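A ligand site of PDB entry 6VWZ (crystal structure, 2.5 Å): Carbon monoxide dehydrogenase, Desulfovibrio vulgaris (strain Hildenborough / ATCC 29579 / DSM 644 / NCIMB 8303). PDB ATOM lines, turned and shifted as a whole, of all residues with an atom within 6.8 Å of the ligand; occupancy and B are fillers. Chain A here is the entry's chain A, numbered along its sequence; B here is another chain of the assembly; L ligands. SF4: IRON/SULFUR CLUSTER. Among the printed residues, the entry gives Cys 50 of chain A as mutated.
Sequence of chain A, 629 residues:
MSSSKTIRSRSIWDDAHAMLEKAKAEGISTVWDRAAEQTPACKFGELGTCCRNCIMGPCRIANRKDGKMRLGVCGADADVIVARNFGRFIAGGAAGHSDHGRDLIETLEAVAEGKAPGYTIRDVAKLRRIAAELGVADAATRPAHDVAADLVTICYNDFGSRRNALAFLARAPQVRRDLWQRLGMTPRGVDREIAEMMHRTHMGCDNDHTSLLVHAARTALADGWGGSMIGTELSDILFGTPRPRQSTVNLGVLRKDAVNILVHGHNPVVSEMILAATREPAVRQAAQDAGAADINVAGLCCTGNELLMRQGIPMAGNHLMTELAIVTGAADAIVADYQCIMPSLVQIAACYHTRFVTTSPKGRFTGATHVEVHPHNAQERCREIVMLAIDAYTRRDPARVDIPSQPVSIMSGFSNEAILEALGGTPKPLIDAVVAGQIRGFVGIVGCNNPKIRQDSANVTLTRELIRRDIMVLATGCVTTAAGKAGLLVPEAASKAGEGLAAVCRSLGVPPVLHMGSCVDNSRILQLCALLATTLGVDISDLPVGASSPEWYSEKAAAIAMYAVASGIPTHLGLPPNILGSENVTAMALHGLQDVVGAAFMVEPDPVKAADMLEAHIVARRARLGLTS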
ATOM      1  N   CYS A  50      -8.732 -17.049 -24.334  1.00  0.00           N
ATOM      2  CA  CYS A  50      -7.610 -17.399 -23.489  1.00  0.00           C
ATOM      3  C   CYS A  50      -6.754 -16.154 -23.289  1.00  0.00           C
ATOM      4  O   CYS A  50      -6.459 -15.439 -24.242  1.00  0.00           O
ATOM      5  CB  CYS A  50      -6.780 -18.521 -24.112  1.00  0.00           C
ATOM      6  SG  CYS A  50      -5.176 -18.814 -23.349  1.00  0.00           S
ATOM      7  N   CYS A  51      -6.354 -15.913 -22.042  1.00  0.00           N
ATOM      8  CA  CYS A  51      -5.546 -14.752 -21.711  1.00  0.00           C
ATOM      9  C   CYS A  51      -4.303 -15.209 -20.957  1.00  0.00           C
ATOM     10  O   CYS A  51      -4.395 -15.987 -20.004  1.00  0.00           O
ATOM     11  CB  CYS A  51      -6.336 -13.750 -20.877  1.00  0.00           C
ATOM     12  SG  CYS A  51      -5.458 -12.207 -20.593  1.00  0.00           S
ATOM     13  N   ARG A  52      -3.143 -14.711 -21.389  1.00  0.00           N
ATOM     14  CA  ARG A  52      -1.862 -15.032 -20.762  1.00  0.00           C
ATOM     15  C   ARG A  52      -1.094 -13.753 -20.419  1.00  0.00           C
ATOM     16  O   ARG A  52       0.139 -13.762 -20.370  1.00  0.00           O
ATOM     17  CB  ARG A  52      -1.028 -15.936 -21.668  1.00  0.00           C
ATOM     18  CG  ARG A  52      -1.730 -17.238 -22.037  1.00  0.00           C
ATOM     19  CD  ARG A  52      -0.992 -17.992 -23.121  1.00  0.00           C
ATOM     20  NE  ARG A  52      -0.796 -17.162 -24.309  1.00  0.00           N
ATOM     21  CZ  ARG A  52      -0.165 -17.569 -25.410  1.00  0.00           C
ATOM     22  NH1 ARG A  52      -0.018 -16.736 -26.437  1.00  0.00           N
ATOM     23  NH2 ARG A  52       0.317 -18.809 -25.483  1.00  0.00           N
ATOM     24  N   ASN A  53      -1.816 -12.657 -20.197  1.00  0.00           N
ATOM     25  CA  ASN A  53      -1.202 -11.345 -20.032  1.00  0.00           C
ATOM     26  C   ASN A  53      -0.633 -11.098 -18.637  1.00  0.00           C
ATOM     27  O   ASN A  53      -0.071 -10.021 -18.397  1.00  0.00           O
ATOM     28  CB  ASN A  53      -2.218 -10.240 -20.380  1.00  0.00           C
ATOM     29  CG  ASN A  53      -2.474 -10.118 -21.870  1.00  0.00           C
ATOM     30  OD1 ASN A  53      -2.179 -11.031 -22.646  1.00  0.00           O
ATOM     31  ND2 ASN A  53      -3.012  -8.981 -22.285  1.00  0.00           N
ATOM     32  N   CYS A  54      -0.774 -12.050 -17.712  1.00  0.00           N
ATOM     33  CA  CYS A  54      -0.133 -11.938 -16.396  1.00  0.00           C
ATOM     34  C   CYS A  54      -0.123 -13.322 -15.764  1.00  0.00           C
ATOM     35  O   CYS A  54      -0.812 -14.232 -16.222  1.00  0.00           O
ATOM     36  CB  CYS A  54      -0.838 -10.911 -15.508  1.00  0.00           C
ATOM     37  SG  CYS A  54      -2.295 -11.537 -14.629  1.00  0.00           S
ATOM     38  N   ILE A  55       0.669 -13.473 -14.707  1.00  0.00           N
ATOM     39  CA  ILE A  55       0.829 -14.766 -14.063  1.00  0.00           C
ATOM     40  C   ILE A  55      -0.079 -14.902 -12.834  1.00  0.00           C
ATOM     41  O   ILE A  55       0.130 -15.793 -12.009  1.00  0.00           O
ATOM     42  CB  ILE A  55       2.294 -15.076 -13.715  1.00  0.00           C
ATOM     43  CG1 ILE A  55       2.825 -14.139 -12.650  1.00  0.00           C
ATOM     44  CG2 ILE A  55       3.160 -15.011 -14.971  1.00  0.00           C
ATOM     45  CD1 ILE A  55       3.840 -14.793 -11.752  1.00  0.00           C
ATOM     46  N   MET A  56      -1.063 -14.021 -12.680  1.00  0.00           N
ATOM     47  CA  MET A  56      -2.260 -14.423 -11.945  1.00  0.00           C
ATOM     48  C   MET A  56      -3.048 -15.435 -12.763  1.00  0.00           C
ATOM     49  O   MET A  56      -3.761 -16.271 -12.197  1.00  0.00           O
ATOM     50  CB  MET A  56      -3.143 -13.218 -11.618  1.00  0.00           C
ATOM     51  CG  MET A  56      -2.673 -12.366 -10.442  1.00  0.00           C
ATOM     52  SD  MET A  56      -3.991 -11.320  -9.779  1.00  0.00           S
ATOM     53  CE  MET A  56      -4.491 -10.401 -11.239  1.00  0.00           C
ATOM     54  N   GLY A  57      -2.911 -15.378 -14.083  1.00  0.00           N
ATOM     55  CA  GLY A  57      -3.401 -16.406 -14.966  1.00  0.00           C
ATOM     56  C   GLY A  57      -2.347 -17.484 -15.166  1.00  0.00           C
ATOM     57  O   GLY A  57      -1.478 -17.684 -14.309  1.00  0.00           O
ATOM     58  N   PRO A  58      -2.392 -18.188 -16.310  1.00  0.00           N
ATOM     59  CA  PRO A  58      -3.302 -18.004 -17.454  1.00  0.00           C
ATOM     60  C   PRO A  58      -4.754 -18.324 -17.122  1.00  0.00           C
ATOM     61  O   PRO A  58      -5.039 -19.166 -16.282  1.00  0.00           O
ATOM     62  CB  PRO A  58      -2.763 -18.984 -18.488  1.00  0.00           C
ATOM     63  CG  PRO A  58      -2.015 -20.004 -17.715  1.00  0.00           C
ATOM     64  CD  PRO A  58      -1.412 -19.260 -16.565  1.00  0.00           C
ATOM     65  N   CYS A  59      -5.660 -17.606 -17.789  1.00  0.00           N
ATOM     66  CA  CYS A  59      -7.086 -17.720 -17.565  1.00  0.00           C
ATOM     67  C   CYS A  59      -7.781 -18.173 -18.840  1.00  0.00           C
ATOM     68  O   CYS A  59      -7.383 -17.807 -19.945  1.00  0.00           O
ATOM     69  CB  CYS A  59      -7.689 -16.388 -17.097  1.00  0.00           C
ATOM     70  SG  CYS A  59      -6.919 -15.745 -15.610  1.00  0.00           S
ATOM     71  N   ARG A  60      -8.836 -18.960 -18.664  1.00  0.00           N
ATOM     72  CA  ARG A  60      -9.697 -19.376 -19.758  1.00  0.00           C
ATOM     73  C   ARG A  60     -11.123 -19.010 -19.413  1.00  0.00           C
ATOM     74  O   ARG A  60     -11.572 -19.237 -18.287  1.00  0.00           O
ATOM     75  CB  ARG A  60      -9.574 -20.884 -19.990  1.00  0.00           C
ATOM     76  CG  ARG A  60      -8.279 -21.322 -20.638  1.00  0.00           C
ATOM     77  CD  ARG A  60      -8.055 -22.814 -20.431  1.00  0.00           C
ATOM     78  NE  ARG A  60      -7.936 -23.137 -19.015  1.00  0.00           N
ATOM     79  CZ  ARG A  60      -7.816 -24.360 -18.522  1.00  0.00           C
ATOM     80  NH1 ARG A  60      -7.813 -25.409 -19.332  1.00  0.00           N
ATOM     81  NH2 ARG A  60      -7.718 -24.535 -17.206  1.00  0.00           N
ATOM     82  N   ILE A  61     -11.835 -18.426 -20.371  1.00  0.00           N
ATOM     83  CA  ILE A  61     -13.257 -18.119 -20.224  1.00  0.00           C
ATOM     84  C   ILE A  61     -14.028 -19.215 -20.944  1.00  0.00           C
ATOM     85  O   ILE A  61     -13.929 -19.357 -22.174  1.00  0.00           O
ATOM     86  CB  ILE A  61     -13.603 -16.731 -20.771  1.00  0.00           C
ATOM     87  CG1 ILE A  61     -12.688 -15.680 -20.152  1.00  0.00           C
ATOM     88  CG2 ILE A  61     -15.057 -16.402 -20.462  1.00  0.00           C
ATOM     89  CD1 ILE A  61     -12.683 -15.676 -18.643  1.00  0.00           C
ATOM     90  N   LEU A  71     -14.975 -15.380 -15.643  1.00  0.00           N
ATOM     91  CA  LEU A  71     -14.100 -14.228 -15.534  1.00  0.00           C
ATOM     92  C   LEU A  71     -12.673 -14.683 -15.284  1.00  0.00           C
ATOM     93  O   LEU A  71     -12.429 -15.769 -14.748  1.00  0.00           O
ATOM     94  CB  LEU A  71     -14.553 -13.290 -14.398  1.00  0.00           C
ATOM     95  CG  LEU A  71     -16.006 -12.830 -14.438  1.00  0.00           C
ATOM     96  CD1 LEU A  71     -16.335 -12.064 -13.171  1.00  0.00           C
ATOM     97  CD2 LEU A  71     -16.264 -11.983 -15.665  1.00  0.00           C
ATOM     98  N   GLY A  72     -11.723 -13.839 -15.674  1.00  0.00           N
ATOM     99  CA  GLY A  72     -10.343 -14.057 -15.310  1.00  0.00           C
ATOM    100  C   GLY A  72     -10.125 -13.791 -13.835  1.00  0.00           C
ATOM    101  O   GLY A  72     -11.020 -13.362 -13.108  1.00  0.00           O
ATOM    102  N   VAL A  73      -8.898 -14.077 -13.374  1.00  0.00           N
ATOM    103  CA  VAL A  73      -8.586 -13.824 -11.976  1.00  0.00           C
ATOM    104  C   VAL A  73      -8.748 -12.349 -11.643  1.00  0.00           C
ATOM    105  O   VAL A  73      -9.235 -11.987 -10.573  1.00  0.00           O
ATOM    106  CB  VAL A  73      -7.169 -14.331 -11.648  1.00  0.00           C
ATOM    107  CG1 VAL A  73      -6.827 -14.027 -10.187  1.00  0.00           C
ATOM    108  CG2 VAL A  73      -7.045 -15.813 -11.934  1.00  0.00           C
ATOM    109  N   CYS A  74      -8.381 -11.467 -12.592  1.00  0.00           N
ATOM    110  CA  CYS A  74      -8.519 -10.031 -12.394  1.00  0.00           C
ATOM    111  C   CYS A  74      -9.956  -9.546 -12.562  1.00  0.00           C
ATOM    112  O   CYS A  74     -10.231  -8.388 -12.242  1.00  0.00           O
ATOM    113  CB  CYS A  74      -7.615  -9.274 -13.370  1.00  0.00           C
ATOM    114  SG  CYS A  74      -8.049  -9.459 -15.121  1.00  0.00           S
ATOM    115  N   GLY A  75     -10.866 -10.390 -13.029  1.00  0.00           N
ATOM    116  CA  GLY A  75     -12.243  -9.993 -13.250  1.00  0.00           C
ATOM    117  C   GLY A  75     -12.624  -9.729 -14.690  1.00  0.00           C
ATOM    118  O   GLY A  75     -13.789  -9.428 -14.947  1.00  0.00           O
ATOM    119  N   ALA A  76     -11.678  -9.834 -15.616  1.00  0.00           N
ATOM    120  CA  ALA A  76     -11.978  -9.542 -17.015  1.00  0.00           C
ATOM    121  C   ALA A  76     -12.906 -10.602 -17.596  1.00  0.00           C
ATOM    122  O   ALA A  76     -12.727 -11.803 -17.357  1.00  0.00           O
ATOM    123  CB  ALA A  76     -10.687  -9.477 -17.834  1.00  0.00           C
ATOM    124  N   ASP A  77     -13.907 -10.160 -18.352  1.00  0.00           N
ATOM    125  CA  ASP A  77     -14.832 -11.072 -19.007  1.00  0.00           C
ATOM    126  C   ASP A  77     -14.330 -11.416 -20.406  1.00  0.00           C
ATOM    127  O   ASP A  77     -13.255 -10.968 -20.838  1.00  0.00           O
ATOM    128  CB  ASP A  77     -16.244 -10.495 -19.035  1.00  0.00           C
ATOM    129  CG  ASP A  77     -16.334  -9.177 -19.798  1.00  0.00           C
ATOM    130  OD1 ASP A  77     -15.400  -8.834 -20.558  1.00  0.00           O
ATOM    131  OD2 ASP A  77     -17.350  -8.471 -19.639  1.00  0.00           O
ATOM    132  N   ILE A  81     -11.124  -9.886 -22.807  1.00  0.00           N
ATOM    133  CA  ILE A  81     -10.030 -10.805 -23.104  1.00  0.00           C
ATOM    134  C   ILE A  81      -9.914 -11.028 -24.611  1.00  0.00           C
ATOM    135  O   ILE A  81      -8.807 -11.033 -25.164  1.00  0.00           O
ATOM    136  CB  ILE A  81     -10.221 -12.133 -22.344  1.00  0.00           C
ATOM    137  CG1 ILE A  81      -9.894 -11.917 -20.861  1.00  0.00           C
ATOM    138  CG2 ILE A  81      -9.368 -13.245 -22.939  1.00  0.00           C
ATOM    139  CD1 ILE A  81     -10.372 -13.030 -19.966  1.00  0.00           C
ATOM    140  N   ARG A  84      -8.654  -7.613 -26.230  1.00  0.00           N
ATOM    141  CA  ARG A  84      -7.233  -7.352 -25.980  1.00  0.00           C
ATOM    142  C   ARG A  84      -6.346  -8.258 -26.832  1.00  0.00           C
ATOM    143  O   ARG A  84      -5.298  -7.819 -27.330  1.00  0.00           O
ATOM    144  CB  ARG A  84      -6.907  -7.525 -24.496  1.00  0.00           C
ATOM    145  CG  ARG A  84      -7.511  -6.454 -23.598  1.00  0.00           C
ATOM    146  CD  ARG A  84      -7.025  -6.565 -22.159  1.00  0.00           C
ATOM    147  NE  ARG A  84      -7.110  -7.940 -21.652  1.00  0.00           N
ATOM    148  CZ  ARG A  84      -7.114  -8.252 -20.353  1.00  0.00           C
ATOM    149  NH1 ARG A  84      -7.040  -7.299 -19.434  1.00  0.00           N
ATOM    150  NH2 ARG A  84      -7.195  -9.528 -19.975  1.00  0.00           N
ATOM    151  N   THR A 201      -3.706  -3.116 -23.472  1.00  0.00           N
ATOM    152  CA  THR A 201      -3.967  -4.536 -23.300  1.00  0.00           C
ATOM    153  C   THR A 201      -3.268  -5.140 -22.083  1.00  0.00           C
ATOM    154  O   THR A 201      -3.416  -6.340 -21.824  1.00  0.00           O
ATOM    155  CB  THR A 201      -3.580  -5.277 -24.575  1.00  0.00           C
ATOM    156  OG1 THR A 201      -2.230  -4.945 -24.929  1.00  0.00           O
ATOM    157  CG2 THR A 201      -4.508  -4.853 -25.704  1.00  0.00           C
ATOM    158  N   HIS A 202      -2.490  -4.344 -21.349  1.00  0.00           N
ATOM    159  CA  HIS A 202      -1.970  -4.754 -20.057  1.00  0.00           C
ATOM    160  C   HIS A 202      -3.115  -4.932 -19.069  1.00  0.00           C
ATOM    161  O   HIS A 202      -4.181  -4.322 -19.206  1.00  0.00           O
ATOM    162  CB  HIS A 202      -0.969  -3.717 -19.543  1.00  0.00           C
ATOM    163  CG  HIS A 202      -0.307  -4.085 -18.254  1.00  0.00           C
ATOM    164  ND1 HIS A 202       0.955  -4.639 -18.191  1.00  0.00           N
ATOM    165  CD2 HIS A 202      -0.705  -3.936 -16.963  1.00  0.00           C
ATOM    166  CE1 HIS A 202       1.294  -4.845 -16.929  1.00  0.00           C
ATOM    167  NE2 HIS A 202       0.297  -4.422 -16.168  1.00  0.00           N
ATOM    168  N   MET A 203      -2.909  -5.791 -18.063  1.00  0.00           N
ATOM    169  CA  MET A 203      -3.928  -6.033 -17.062  1.00  0.00           C
ATOM    170  C   MET A 203      -4.350  -4.731 -16.400  1.00  0.00           C
ATOM    171  O   MET A 203      -3.521  -3.894 -16.051  1.00  0.00           O
ATOM    172  CB  MET A 203      -3.429  -7.007 -15.990  1.00  0.00           C
ATOM    173  CG  MET A 203      -4.517  -7.490 -14.996  1.00  0.00           C
ATOM    174  SD  MET A 203      -5.153  -6.290 -13.761  1.00  0.00           S
ATOM    175  CE  MET A 203      -4.390  -6.845 -12.238  1.00  0.00           C
ATOM    176  N   GLY A 204      -5.663  -4.563 -16.229  1.00  0.00           N
ATOM    177  CA  GLY A 204      -6.184  -3.445 -15.461  1.00  0.00           C
ATOM    178  C   GLY A 204      -5.964  -2.088 -16.082  1.00  0.00           C
ATOM    179  O   GLY A 204      -5.896  -1.091 -15.347  1.00  0.00           O
ATOM    180  N   GLN B  38      -9.868 -20.758 -11.738  1.00  0.00           N
ATOM    181  CA  GLN B  38      -8.912 -20.904 -12.819  1.00  0.00           C
ATOM    182  C   GLN B  38      -7.820 -21.927 -12.504  1.00  0.00           C
ATOM    183  O   GLN B  38      -6.845 -22.022 -13.258  1.00  0.00           O
ATOM    184  CB  GLN B  38      -8.293 -19.535 -13.145  1.00  0.00           C
ATOM    185  CG  GLN B  38      -9.274 -18.535 -13.730  1.00  0.00           C
ATOM    186  CD  GLN B  38      -9.797 -18.941 -15.106  1.00  0.00           C
ATOM    187  OE1 GLN B  38      -9.164 -19.713 -15.820  1.00  0.00           O
ATOM    188  NE2 GLN B  38     -10.960 -18.407 -15.479  1.00  0.00           N
ATOM    189  N   PRO B 343     -10.882  -5.024 -13.097  1.00  0.00           N
ATOM    190  CA  PRO B 343     -12.244  -4.634 -13.486  1.00  0.00           C
ATOM    191  C   PRO B 343     -13.344  -5.180 -12.594  1.00  0.00           C
ATOM    192  O   PRO B 343     -14.491  -4.741 -12.718  1.00  0.00           O
ATOM    193  CB  PRO B 343     -12.372  -5.188 -14.920  1.00  0.00           C
ATOM    194  CG  PRO B 343     -11.349  -6.276 -14.999  1.00  0.00           C
ATOM    195  CD  PRO B 343     -10.206  -5.825 -14.133  1.00  0.00           C
ATOM    196  N   TYR B 553       3.039 -10.449 -10.357  1.00  0.00           N
ATOM    197  CA  TYR B 553       2.102 -11.017 -11.326  1.00  0.00           C
ATOM    198  C   TYR B 553       2.148 -10.361 -12.707  1.00  0.00           C
ATOM    199  O   TYR B 553       1.855 -11.040 -13.698  1.00  0.00           O
ATOM    200  CB  TYR B 553       0.663 -10.940 -10.812  1.00  0.00           C
ATOM    201  CG  TYR B 553       0.052  -9.567 -10.951  1.00  0.00           C
ATOM    202  CD1 TYR B 553       0.215  -8.616  -9.958  1.00  0.00           C
ATOM    203  CD2 TYR B 553      -0.655  -9.204 -12.092  1.00  0.00           C
ATOM    204  CE1 TYR B 553      -0.315  -7.357 -10.073  1.00  0.00           C
ATOM    205  CE2 TYR B 553      -1.183  -7.939 -12.228  1.00  0.00           C
ATOM    206  CZ  TYR B 553      -1.007  -7.019 -11.210  1.00  0.00           C
ATOM    207  OH  TYR B 553      -1.537  -5.760 -11.325  1.00  0.00           O
HETATM  208 FE1  SF4 L   1      -5.513 -12.129 -18.327  1.00  0.00          FE
HETATM  209 FE2  SF4 L   1      -6.145 -13.671 -16.162  1.00  0.00          FE
HETATM  210 FE3  SF4 L   1      -6.668 -10.987 -16.115  1.00  0.00          FE
HETATM  211 FE4  SF4 L   1      -4.071 -11.881 -16.009  1.00  0.00          FE
HETATM  212  S1  SF4 L   1      -5.717 -12.231 -14.456  1.00  0.00           S
HETATM  213  S2  SF4 L   1      -4.879 -10.185 -17.304  1.00  0.00           S
HETATM  214  S3  SF4 L   1      -4.196 -13.712 -17.358  1.00  0.00           S
HETATM  215  S4  SF4 L   1      -7.600 -12.539 -17.503  1.00  0.00           S
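SG of Cys 54 is bound to FE4 of the ligand (2.3 Å). SG of Cys 59 binds FE2 of the ligand, 2.3 Å away. A sulfur (S1) of the ligand sits close to the backbone NH (N) of Cys 74 (3.3 Å). The side-chain sulfur (SG) of Cys 74 binds an iron atom (FE3) of the ligand. The side-chain sulfur of Cys 51 binds an iron atom (FE1) of the ligand, 2.3 Å away. NH2 of Arg 84 sits close to S2 of the ligand (3.6 Å).
Asn 53 touches the ligand. Met 56 touches the ligand. CA of Gly 57 touches S3 of the ligand, 3.7 Å away. Gly 72 touches the ligand. Val 73 touches the ligand (CB to S1, 3.8 Å). CD1 of Ile 81 touches S4 of the ligand, at 3.7 Å. CG of Met 203 touches S2 of the ligand, at 3.6 Å. Hydrophobic or aromatic side chains within 4 Å of the ligand: Met 56, Val 73, Ile 81 and Met 203.
N of Cys 51 lies within hydrogen-bond range of O of Cys 59 (3.0 Å). The backbone NH of Met 56 lies close to the side-chain sulfur of Cys 54 (3.4 Å). N of Asn 53 lies close to SG of Cys 51 (3.7 Å). The side-chain sulfur (SG) of Cys 59 sits close to the backbone NH (N) of Val 73 (3.4 Å). ND2 of Asn 53 sits at hydrogen-bond distance from O of Thr 201 (2.7 Å). N of Ala 76 lies close to SG of Cys 74 (3.7 Å). The side-chain sulfur (SG) of Cys 51 lies close to the guanidinium group (NH2) of Arg 84 (3.3 Å).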
